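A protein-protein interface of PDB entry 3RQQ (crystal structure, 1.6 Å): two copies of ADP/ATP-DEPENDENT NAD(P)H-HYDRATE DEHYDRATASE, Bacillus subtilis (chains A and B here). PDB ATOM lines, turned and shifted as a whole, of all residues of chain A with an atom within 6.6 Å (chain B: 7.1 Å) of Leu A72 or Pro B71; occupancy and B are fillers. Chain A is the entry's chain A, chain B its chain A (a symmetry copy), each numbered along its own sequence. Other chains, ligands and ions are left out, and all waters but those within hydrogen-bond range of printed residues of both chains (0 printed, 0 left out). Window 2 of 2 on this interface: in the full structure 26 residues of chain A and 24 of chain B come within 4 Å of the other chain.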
ATOM      1  N   PRO A  43     -32.839 -23.016 -13.094  1.00  0.00           N
ATOM      2  CA  PRO A  43     -32.632 -21.568 -12.976  1.00  0.00           C
ATOM      3  C   PRO A  43     -32.185 -20.894 -14.260  1.00  0.00           C
ATOM      4  O   PRO A  43     -32.495 -19.725 -14.534  1.00  0.00           O
ATOM      5  CB  PRO A  43     -31.505 -21.467 -11.935  1.00  0.00           C
ATOM      6  CG  PRO A  43     -30.795 -22.826 -12.020  1.00  0.00           C
ATOM      7  CD  PRO A  43     -31.884 -23.793 -12.292  1.00  0.00           C
ATOM      8  N   GLY A  44     -31.400 -21.624 -15.072  1.00  0.00           N
ATOM      9  CA  GLY A  44     -30.723 -21.012 -16.222  1.00  0.00           C
ATOM     10  C   GLY A  44     -31.660 -20.430 -17.267  1.00  0.00           C
ATOM     11  O   GLY A  44     -31.338 -19.412 -17.924  1.00  0.00           O
ATOM     12  N   LEU A  47     -32.176 -16.684 -17.005  1.00  0.00           N
ATOM     13  CA  LEU A  47     -31.076 -15.879 -17.518  1.00  0.00           C
ATOM     14  C   LEU A  47     -31.116 -15.846 -19.057  1.00  0.00           C
ATOM     15  O   LEU A  47     -30.939 -14.769 -19.663  1.00  0.00           O
ATOM     16  CB  LEU A  47     -29.720 -16.393 -17.005  1.00  0.00           C
ATOM     17  CG  LEU A  47     -28.487 -15.618 -17.468  1.00  0.00           C
ATOM     18  CD1 LEU A  47     -28.623 -14.069 -17.306  1.00  0.00           C
ATOM     19  CD2 LEU A  47     -27.224 -16.126 -16.735  1.00  0.00           C
ATOM     20  N   ASN A  68     -34.351 -17.451  -5.059  1.00  0.00           N
ATOM     21  CA  ASN A  68     -32.979 -17.944  -5.146  1.00  0.00           C
ATOM     22  C   ASN A  68     -32.309 -17.850  -6.519  1.00  0.00           C
ATOM     23  O   ASN A  68     -31.095 -18.021  -6.623  1.00  0.00           O
ATOM     24  CB  ASN A  68     -32.897 -19.369  -4.598  1.00  0.00           C
ATOM     25  CG  ASN A  68     -33.205 -19.426  -3.113  1.00  0.00           C
ATOM     26  OD1 ASN A  68     -33.024 -18.445  -2.378  1.00  0.00           O
ATOM     27  ND2 ASN A  68     -33.721 -20.571  -2.666  1.00  0.00           N
ATOM     28  N   VAL A  69     -33.100 -17.607  -7.545  1.00  0.00           N
ATOM     29  CA  VAL A  69     -32.598 -17.439  -8.909  1.00  0.00           C
ATOM     30  C   VAL A  69     -32.143 -16.017  -9.168  1.00  0.00           C
ATOM     31  O   VAL A  69     -31.211 -15.774  -9.954  1.00  0.00           O
ATOM     32  CB  VAL A  69     -33.636 -17.906  -9.909  1.00  0.00           C
ATOM     33  CG1 VAL A  69     -33.110 -17.771 -11.403  1.00  0.00           C
ATOM     34  CG2 VAL A  69     -34.048 -19.394  -9.631  1.00  0.00           C
ATOM     35  N   ILE A  70     -32.765 -15.036  -8.514  1.00  0.00           N
ATOM     36  CA  ILE A  70     -32.389 -13.640  -8.710  1.00  0.00           C
ATOM     37  C   ILE A  70     -30.876 -13.396  -8.657  1.00  0.00           C
ATOM     38  O   ILE A  70     -30.355 -12.777  -9.567  1.00  0.00           O
ATOM     39  CB  ILE A  70     -33.133 -12.733  -7.695  1.00  0.00           C
ATOM     40  CG1 ILE A  70     -34.630 -12.756  -8.001  1.00  0.00           C
ATOM     41  CG2 ILE A  70     -32.631 -11.288  -7.777  1.00  0.00           C
ATOM     42  CD1 ILE A  70     -35.482 -11.993  -6.917  1.00  0.00           C
ATOM     43  N   PRO A  71     -30.170 -13.833  -7.612  1.00  0.00           N
ATOM     44  CA  PRO A  71     -28.718 -13.541  -7.526  1.00  0.00           C
ATOM     45  C   PRO A  71     -27.898 -14.140  -8.671  1.00  0.00           C
ATOM     46  O   PRO A  71     -26.764 -13.685  -8.932  1.00  0.00           O
ATOM     47  CB  PRO A  71     -28.338 -14.086  -6.186  1.00  0.00           C
ATOM     48  CG  PRO A  71     -29.371 -14.997  -5.817  1.00  0.00           C
ATOM     49  CD  PRO A  71     -30.624 -14.531  -6.402  1.00  0.00           C
ATOM     50  N   LEU A  72     -28.445 -15.142  -9.361  1.00  0.00           N
ATOM     51  CA  LEU A  72     -27.739 -15.778 -10.483  1.00  0.00           C
ATOM     52  C   LEU A  72     -27.844 -14.987 -11.789  1.00  0.00           C
ATOM     53  O   LEU A  72     -27.051 -15.187 -12.721  1.00  0.00           O
ATOM     54  CB  LEU A  72     -28.258 -17.208 -10.704  1.00  0.00           C
ATOM     55  CG  LEU A  72     -28.418 -17.966  -9.396  1.00  0.00           C
ATOM     56  CD1 LEU A  72     -28.932 -19.421  -9.672  1.00  0.00           C
ATOM     57  CD2 LEU A  72     -27.144 -18.003  -8.590  1.00  0.00           C
ATOM     58  N   ILE A  73     -28.837 -14.112 -11.865  1.00  0.00           N
ATOM     59  CA  ILE A  73     -29.095 -13.304 -13.039  1.00  0.00           C
ATOM     60  C   ILE A  73     -28.368 -11.978 -12.959  1.00  0.00           C
ATOM     61  O   ILE A  73     -27.780 -11.526 -13.926  1.00  0.00           O
ATOM     62  CB  ILE A  73     -30.625 -13.042 -13.236  1.00  0.00           C
ATOM     63  CG1 ILE A  73     -31.363 -14.362 -13.430  1.00  0.00           C
ATOM     64  CG2 ILE A  73     -30.847 -12.100 -14.427  1.00  0.00           C
ATOM     65  CD1 ILE A  73     -32.873 -14.195 -13.309  1.00  0.00           C
ATOM     66  N   VAL A  74     -28.391 -11.355 -11.790  1.00  0.00           N
ATOM     67  CA  VAL A  74     -27.899  -9.984 -11.622  1.00  0.00           C
ATOM     68  C   VAL A  74     -26.512  -9.690 -12.222  1.00  0.00           C
ATOM     69  O   VAL A  74     -26.339  -8.727 -12.947  1.00  0.00           O
ATOM     70  CB  VAL A  74     -27.974  -9.528 -10.158  1.00  0.00           C
ATOM     71  CG1 VAL A  74     -27.382  -8.116  -9.973  1.00  0.00           C
ATOM     72  CG2 VAL A  74     -29.437  -9.541  -9.675  1.00  0.00           C
ATOM     73  N   PRO A  75     -25.499 -10.526 -11.957  1.00  0.00           N
ATOM     74  CA  PRO A  75     -24.156 -10.184 -12.432  1.00  0.00           C
ATOM     75  C   PRO A  75     -24.045 -10.201 -13.936  1.00  0.00           C
ATOM     76  O   PRO A  75     -23.173  -9.468 -14.505  1.00  0.00           O
ATOM     77  CB  PRO A  75     -23.261 -11.266 -11.815  1.00  0.00           C
ATOM     78  CG  PRO A  75     -24.085 -11.914 -10.783  1.00  0.00           C
ATOM     79  CD  PRO A  75     -25.508 -11.675 -11.019  1.00  0.00           C
ATOM     80  N   VAL A  76     -24.912 -10.967 -14.586  1.00  0.00           N
ATOM     81  CA  VAL A  76     -24.887 -11.097 -16.056  1.00  0.00           C
ATOM     82  C   VAL A  76     -25.844 -10.088 -16.742  1.00  0.00           C
ATOM     83  O   VAL A  76     -25.495  -9.536 -17.828  1.00  0.00           O
ATOM     84  CB  VAL A  76     -25.217 -12.524 -16.483  1.00  0.00           C
ATOM     85  CG1 VAL A  76     -25.165 -12.634 -17.982  1.00  0.00           C
ATOM     86  CG2 VAL A  76     -24.257 -13.525 -15.785  1.00  0.00           C
ATOM     87  N   LEU A  77     -26.939  -9.748 -16.054  1.00  0.00           N
ATOM     88  CA  LEU A  77     -27.989  -8.927 -16.612  1.00  0.00           C
ATOM     89  C   LEU A  77     -28.432  -7.904 -15.550  1.00  0.00           C
ATOM     90  O   LEU A  77     -29.556  -7.984 -15.001  1.00  0.00           O
ATOM     91  CB  LEU A  77     -29.128  -9.796 -17.110  1.00  0.00           C
ATOM     92  CG  LEU A  77     -30.220  -9.091 -17.906  1.00  0.00           C
ATOM     93  CD1 LEU A  77     -29.726  -8.484 -19.225  1.00  0.00           C
ATOM     94  CD2 LEU A  77     -31.431 -10.039 -18.128  1.00  0.00           C
ATOM     95  N   TYR A  82     -36.803  -7.022 -10.736  1.00  0.00           N
ATOM     96  CA  TYR A  82     -37.373  -8.304 -10.249  1.00  0.00           C
ATOM     97  C   TYR A  82     -38.723  -8.122  -9.578  1.00  0.00           C
ATOM     98  O   TYR A  82     -38.967  -7.102  -8.905  1.00  0.00           O
ATOM     99  CB  TYR A  82     -36.374  -9.006  -9.276  1.00  0.00           C
ATOM    100  CG  TYR A  82     -35.095  -9.263  -9.967  1.00  0.00           C
ATOM    101  CD1 TYR A  82     -34.951 -10.354 -10.807  1.00  0.00           C
ATOM    102  CD2 TYR A  82     -34.056  -8.357  -9.872  1.00  0.00           C
ATOM    103  CE1 TYR A  82     -33.830 -10.535 -11.532  1.00  0.00           C
ATOM    104  CE2 TYR A  82     -32.947  -8.488 -10.681  1.00  0.00           C
ATOM    105  CZ  TYR A  82     -32.797  -9.613 -11.436  1.00  0.00           C
ATOM    106  OH  TYR A  82     -31.703  -9.792 -12.259  1.00  0.00           O
ATOM    107  N   THR B  65     -24.264 -32.046  -9.209  1.00  0.00           N
ATOM    108  CA  THR B  65     -23.249 -31.479  -8.351  1.00  0.00           C
ATOM    109  C   THR B  65     -23.850 -31.188  -6.971  1.00  0.00           C
ATOM    110  O   THR B  65     -25.053 -31.234  -6.759  1.00  0.00           O
ATOM    111  CB  THR B  65     -22.630 -30.220  -8.973  1.00  0.00           C
ATOM    112  OG1 THR B  65     -21.469 -29.826  -8.220  1.00  0.00           O
ATOM    113  CG2 THR B  65     -23.638 -29.057  -8.994  1.00  0.00           C
ATOM    114  N   SER B  66     -22.981 -30.874  -6.014  1.00  0.00           N
ATOM    115  CA  SER B  66     -23.428 -30.476  -4.715  1.00  0.00           C
ATOM    116  C   SER B  66     -24.304 -29.246  -4.790  1.00  0.00           C
ATOM    117  O   SER B  66     -24.071 -28.333  -5.579  1.00  0.00           O
ATOM    118  CB  SER B  66     -22.190 -30.227  -3.792  1.00  0.00           C
ATOM    119  OG  SER B  66     -21.521 -31.462  -3.513  1.00  0.00           O
ATOM    120  N   GLU B  67     -25.347 -29.204  -3.969  1.00  0.00           N
ATOM    121  CA  GLU B  67     -26.280 -28.107  -3.954  1.00  0.00           C
ATOM    122  C   GLU B  67     -25.633 -26.720  -3.954  1.00  0.00           C
ATOM    123  O   GLU B  67     -26.048 -25.835  -4.683  1.00  0.00           O
ATOM    124  CB  GLU B  67     -27.219 -28.255  -2.752  1.00  0.00           C
ATOM    125  CG  GLU B  67     -27.978 -27.084  -2.371  1.00  0.00           C
ATOM    126  CD  GLU B  67     -29.144 -27.486  -1.425  1.00  0.00           C
ATOM    127  OE1 GLU B  67     -28.895 -28.085  -0.352  1.00  0.00           O
ATOM    128  OE2 GLU B  67     -30.295 -27.237  -1.801  1.00  0.00           O
ATOM    129  N   ASN B  68     -24.602 -26.520  -3.132  1.00  0.00           N
ATOM    130  CA  ASN B  68     -23.942 -25.221  -3.046  1.00  0.00           C
ATOM    131  C   ASN B  68     -23.085 -24.814  -4.248  1.00  0.00           C
ATOM    132  O   ASN B  68     -22.693 -23.653  -4.358  1.00  0.00           O
ATOM    133  CB  ASN B  68     -23.138 -25.124  -1.749  1.00  0.00           C
ATOM    134  CG  ASN B  68     -24.032 -25.152  -0.523  1.00  0.00           C
ATOM    135  OD1 ASN B  68     -25.213 -24.780  -0.576  1.00  0.00           O
ATOM    136  ND2 ASN B  68     -23.485 -25.643   0.589  1.00  0.00           N
ATOM    137  N   VAL B  69     -22.790 -25.766  -5.111  1.00  0.00           N
ATOM    138  CA  VAL B  69     -22.024 -25.517  -6.332  1.00  0.00           C
ATOM    139  C   VAL B  69     -22.911 -25.035  -7.462  1.00  0.00           C
ATOM    140  O   VAL B  69     -22.481 -24.252  -8.327  1.00  0.00           O
ATOM    141  CB  VAL B  69     -21.227 -26.749  -6.708  1.00  0.00           C
ATOM    142  CG1 VAL B  69     -20.353 -26.504  -8.014  1.00  0.00           C
ATOM    143  CG2 VAL B  69     -20.292 -27.190  -5.528  1.00  0.00           C
ATOM    144  N   ILE B  70     -24.173 -25.464  -7.489  1.00  0.00           N
ATOM    145  CA  ILE B  70     -25.090 -25.049  -8.544  1.00  0.00           C
ATOM    146  C   ILE B  70     -25.069 -23.540  -8.820  1.00  0.00           C
ATOM    147  O   ILE B  70     -24.926 -23.163  -9.969  1.00  0.00           O
ATOM    148  CB  ILE B  70     -26.529 -25.535  -8.231  1.00  0.00           C
ATOM    149  CG1 ILE B  70     -26.569 -27.062  -8.290  1.00  0.00           C
ATOM    150  CG2 ILE B  70     -27.534 -24.972  -9.242  1.00  0.00           C
ATOM    151  CD1 ILE B  70     -27.954 -27.650  -7.822  1.00  0.00           C
ATOM    152  N   PRO B  71     -25.238 -22.680  -7.815  1.00  0.00           N
ATOM    153  CA  PRO B  71     -25.284 -21.222  -8.088  1.00  0.00           C
ATOM    154  C   PRO B  71     -23.996 -20.667  -8.701  1.00  0.00           C
ATOM    155  O   PRO B  71     -24.015 -19.576  -9.310  1.00  0.00           O
ATOM    156  CB  PRO B  71     -25.598 -20.633  -6.750  1.00  0.00           C
ATOM    157  CG  PRO B  71     -25.270 -21.632  -5.786  1.00  0.00           C
ATOM    158  CD  PRO B  71     -25.488 -22.941  -6.391  1.00  0.00           C
ATOM    159  N   LEU B  72     -22.886 -21.392  -8.560  1.00  0.00           N
ATOM    160  CA  LEU B  72     -21.601 -20.946  -9.120  1.00  0.00           C
ATOM    161  C   LEU B  72     -21.457 -21.245 -10.614  1.00  0.00           C
ATOM    162  O   LEU B  72     -20.614 -20.653 -11.304  1.00  0.00           O
ATOM    163  CB  LEU B  72     -20.431 -21.581  -8.352  1.00  0.00           C
ATOM    164  CG  LEU B  72     -20.645 -21.540  -6.848  1.00  0.00           C
ATOM    165  CD1 LEU B  72     -19.421 -22.182  -6.108  1.00  0.00           C
ATOM    166  CD2 LEU B  72     -20.892 -20.143  -6.337  1.00  0.00           C
ATOM    167  N   ILE B  73     -22.258 -22.181 -11.103  1.00  0.00           N
ATOM    168  CA  ILE B  73     -22.231 -22.605 -12.488  1.00  0.00           C
ATOM    169  C   ILE B  73     -23.202 -21.797 -13.324  1.00  0.00           C
ATOM    170  O   ILE B  73     -22.883 -21.373 -14.421  1.00  0.00           O
ATOM    171  CB  ILE B  73     -22.566 -24.126 -12.634  1.00  0.00           C
ATOM    172  CG1 ILE B  73     -21.533 -24.964 -11.890  1.00  0.00           C
ATOM    173  CG2 ILE B  73     -22.627 -24.509 -14.118  1.00  0.00           C
ATOM    174  CD1 ILE B  73     -21.980 -26.412 -11.732  1.00  0.00           C
ATOM    175  N   VAL B  74     -24.394 -21.565 -12.795  1.00  0.00           N
ATOM    176  CA  VAL B  74     -25.491 -20.969 -13.565  1.00  0.00           C
ATOM    177  C   VAL B  74     -25.139 -19.703 -14.366  1.00  0.00           C
ATOM    178  O   VAL B  74     -25.433 -19.612 -15.545  1.00  0.00           O
ATOM    179  CB  VAL B  74     -26.737 -20.744 -12.697  1.00  0.00           C
ATOM    180  CG1 VAL B  74     -27.861 -20.045 -13.490  1.00  0.00           C
ATOM    181  CG2 VAL B  74     -27.253 -22.089 -12.152  1.00  0.00           C
ATOM    182  N   PRO B  75     -24.479 -18.711 -13.756  1.00  0.00           N
ATOM    183  CA  PRO B  75     -24.246 -17.462 -14.485  1.00  0.00           C
ATOM    184  C   PRO B  75     -23.314 -17.634 -15.659  1.00  0.00           C
ATOM    185  O   PRO B  75     -23.408 -16.841 -16.651  1.00  0.00           O
ATOM    186  CB  PRO B  75     -23.622 -16.534 -13.436  1.00  0.00           C
ATOM    187  CG  PRO B  75     -23.864 -17.188 -12.141  1.00  0.00           C
ATOM    188  CD  PRO B  75     -24.140 -18.614 -12.315  1.00  0.00           C
ATOM    189  N   VAL B  76     -22.464 -18.651 -15.597  1.00  0.00           N
ATOM    190  CA  VAL B  76     -21.478 -18.907 -16.665  1.00  0.00           C
ATOM    191  C   VAL B  76     -22.013 -19.913 -17.716  1.00  0.00           C
ATOM    192  O   VAL B  76     -21.740 -19.741 -18.942  1.00  0.00           O
ATOM    193  CB  VAL B  76     -20.156 -19.396 -16.081  1.00  0.00           C
ATOM    194  CG1 VAL B  76     -19.164 -19.630 -17.187  1.00  0.00           C
ATOM    195  CG2 VAL B  76     -19.633 -18.384 -15.025  1.00  0.00           C
ATOM    196  N   TYR B  82     -29.782 -29.361 -13.720  1.00  0.00           N
ATOM    197  CA  TYR B  82     -29.160 -29.906 -12.486  1.00  0.00           C
ATOM    198  C   TYR B  82     -29.922 -31.094 -11.927  1.00  0.00           C
ATOM    199  O   TYR B  82     -31.164 -31.147 -12.004  1.00  0.00           O
ATOM    200  CB  TYR B  82     -29.030 -28.786 -11.404  1.00  0.00           C
ATOM    201  CG  TYR B  82     -28.208 -27.676 -11.926  1.00  0.00           C
ATOM    202  CD1 TYR B  82     -26.826 -27.756 -11.923  1.00  0.00           C
ATOM    203  CD2 TYR B  82     -28.809 -26.585 -12.526  1.00  0.00           C
ATOM    204  CE1 TYR B  82     -26.069 -26.802 -12.500  1.00  0.00           C
ATOM    205  CE2 TYR B  82     -28.043 -25.656 -13.197  1.00  0.00           C
ATOM    206  CZ  TYR B  82     -26.684 -25.717 -13.108  1.00  0.00           C
ATOM    207  OH  TYR B  82     -25.875 -24.807 -13.759  1.00  0.00           O
ATOM    208  N   ARG B  84     -29.836 -32.100  -8.226  1.00  0.00           N
ATOM    209  CA  ARG B  84     -29.305 -31.542  -7.000  1.00  0.00           C
ATOM    210  C   ARG B  84     -28.688 -32.633  -6.125  1.00  0.00           C
ATOM    211  O   ARG B  84     -29.336 -33.638  -5.815  1.00  0.00           O
ATOM    212  CB  ARG B  84     -30.460 -30.789  -6.274  1.00  0.00           C
ATOM    213  CG  ARG B  84     -30.103 -30.128  -5.029  1.00  0.00           C
ATOM    214  CD  ARG B  84     -31.367 -29.252  -4.511  1.00  0.00           C
ATOM    215  NE  ARG B  84     -31.714 -28.226  -5.509  1.00  0.00           N
ATOM    216  CZ  ARG B  84     -31.186 -27.000  -5.559  1.00  0.00           C
ATOM    217  NH1 ARG B  84     -30.432 -26.547  -4.573  1.00  0.00           N
ATOM    218  NH2 ARG B  84     -31.464 -26.177  -6.583  1.00  0.00           N
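Val B74 touches Pro A43. Leu A47 touches Pro B75. Leu A72 touches Pro B71. CD1 of Leu A72 touches CB of Val B74, 3.96 Å away. O of Leu A72 touches CB of Pro B75, 3.8 Å away. Val A76 touches Pro B75.
Of the printed residues of chain B, Pro A43 touches Val B74 (3.6 Å). Of the printed residues of chain B, Leu A47 touches Pro B75 (3.9 Å). Leu A72 touches just these residues of chain B: Pro B71 (3.6 Å), Val B74 (3.96 Å) and Pro B75 (3.8 Å). Ile A73 touches none of the printed residues of chain B. Pro B71 touches just one residue of chain A: Leu A72 (3.6 Å). Of the printed residues of chain A, Val B74 touches Pro A43 and Leu A72. The nearest residue of chain A that does not touch Pro B71 is Asn A68 (6.1 Å). The nearest printed residue of chain B that does not touch Val A76 is Val B76 (5.4 Å).
Of the 14 printed residues of chain B, 3 touch a printed residue of chain A. Printed residues of chain B that touch a printed residue of chain A: Pro B71, Val B74 and Pro B75. Hydrophobic or aromatic side chains of chain B within 4 Å of the printed part of chain A: Pro B71, Val B74 and Pro B75. Hydrophobic or aromatic side chains of chain A within 4 Å of the printed part of chain B: Pro A43, Leu A47, Leu A72 and Val A76.
Leu A72 touches Pro B71, but with the chains exchanged Pro A71 does not touch Leu B72 (8.6 Å). Leu A72 touches Val B74, but with the chains exchanged Val A74 does not touch Leu B72 (11.9 Å). Leu A72 touches Pro B75, but with the chains exchanged Pro A75 does not touch Leu B72 (9.4 Å). Val A76 touches Pro B75, but with the chains exchanged Pro A75 does not touch Val B76 (8.3 Å). Positions printed for both chains: 68, 69, 70, 71, 72, 73, 74, 75, 76 and 82.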
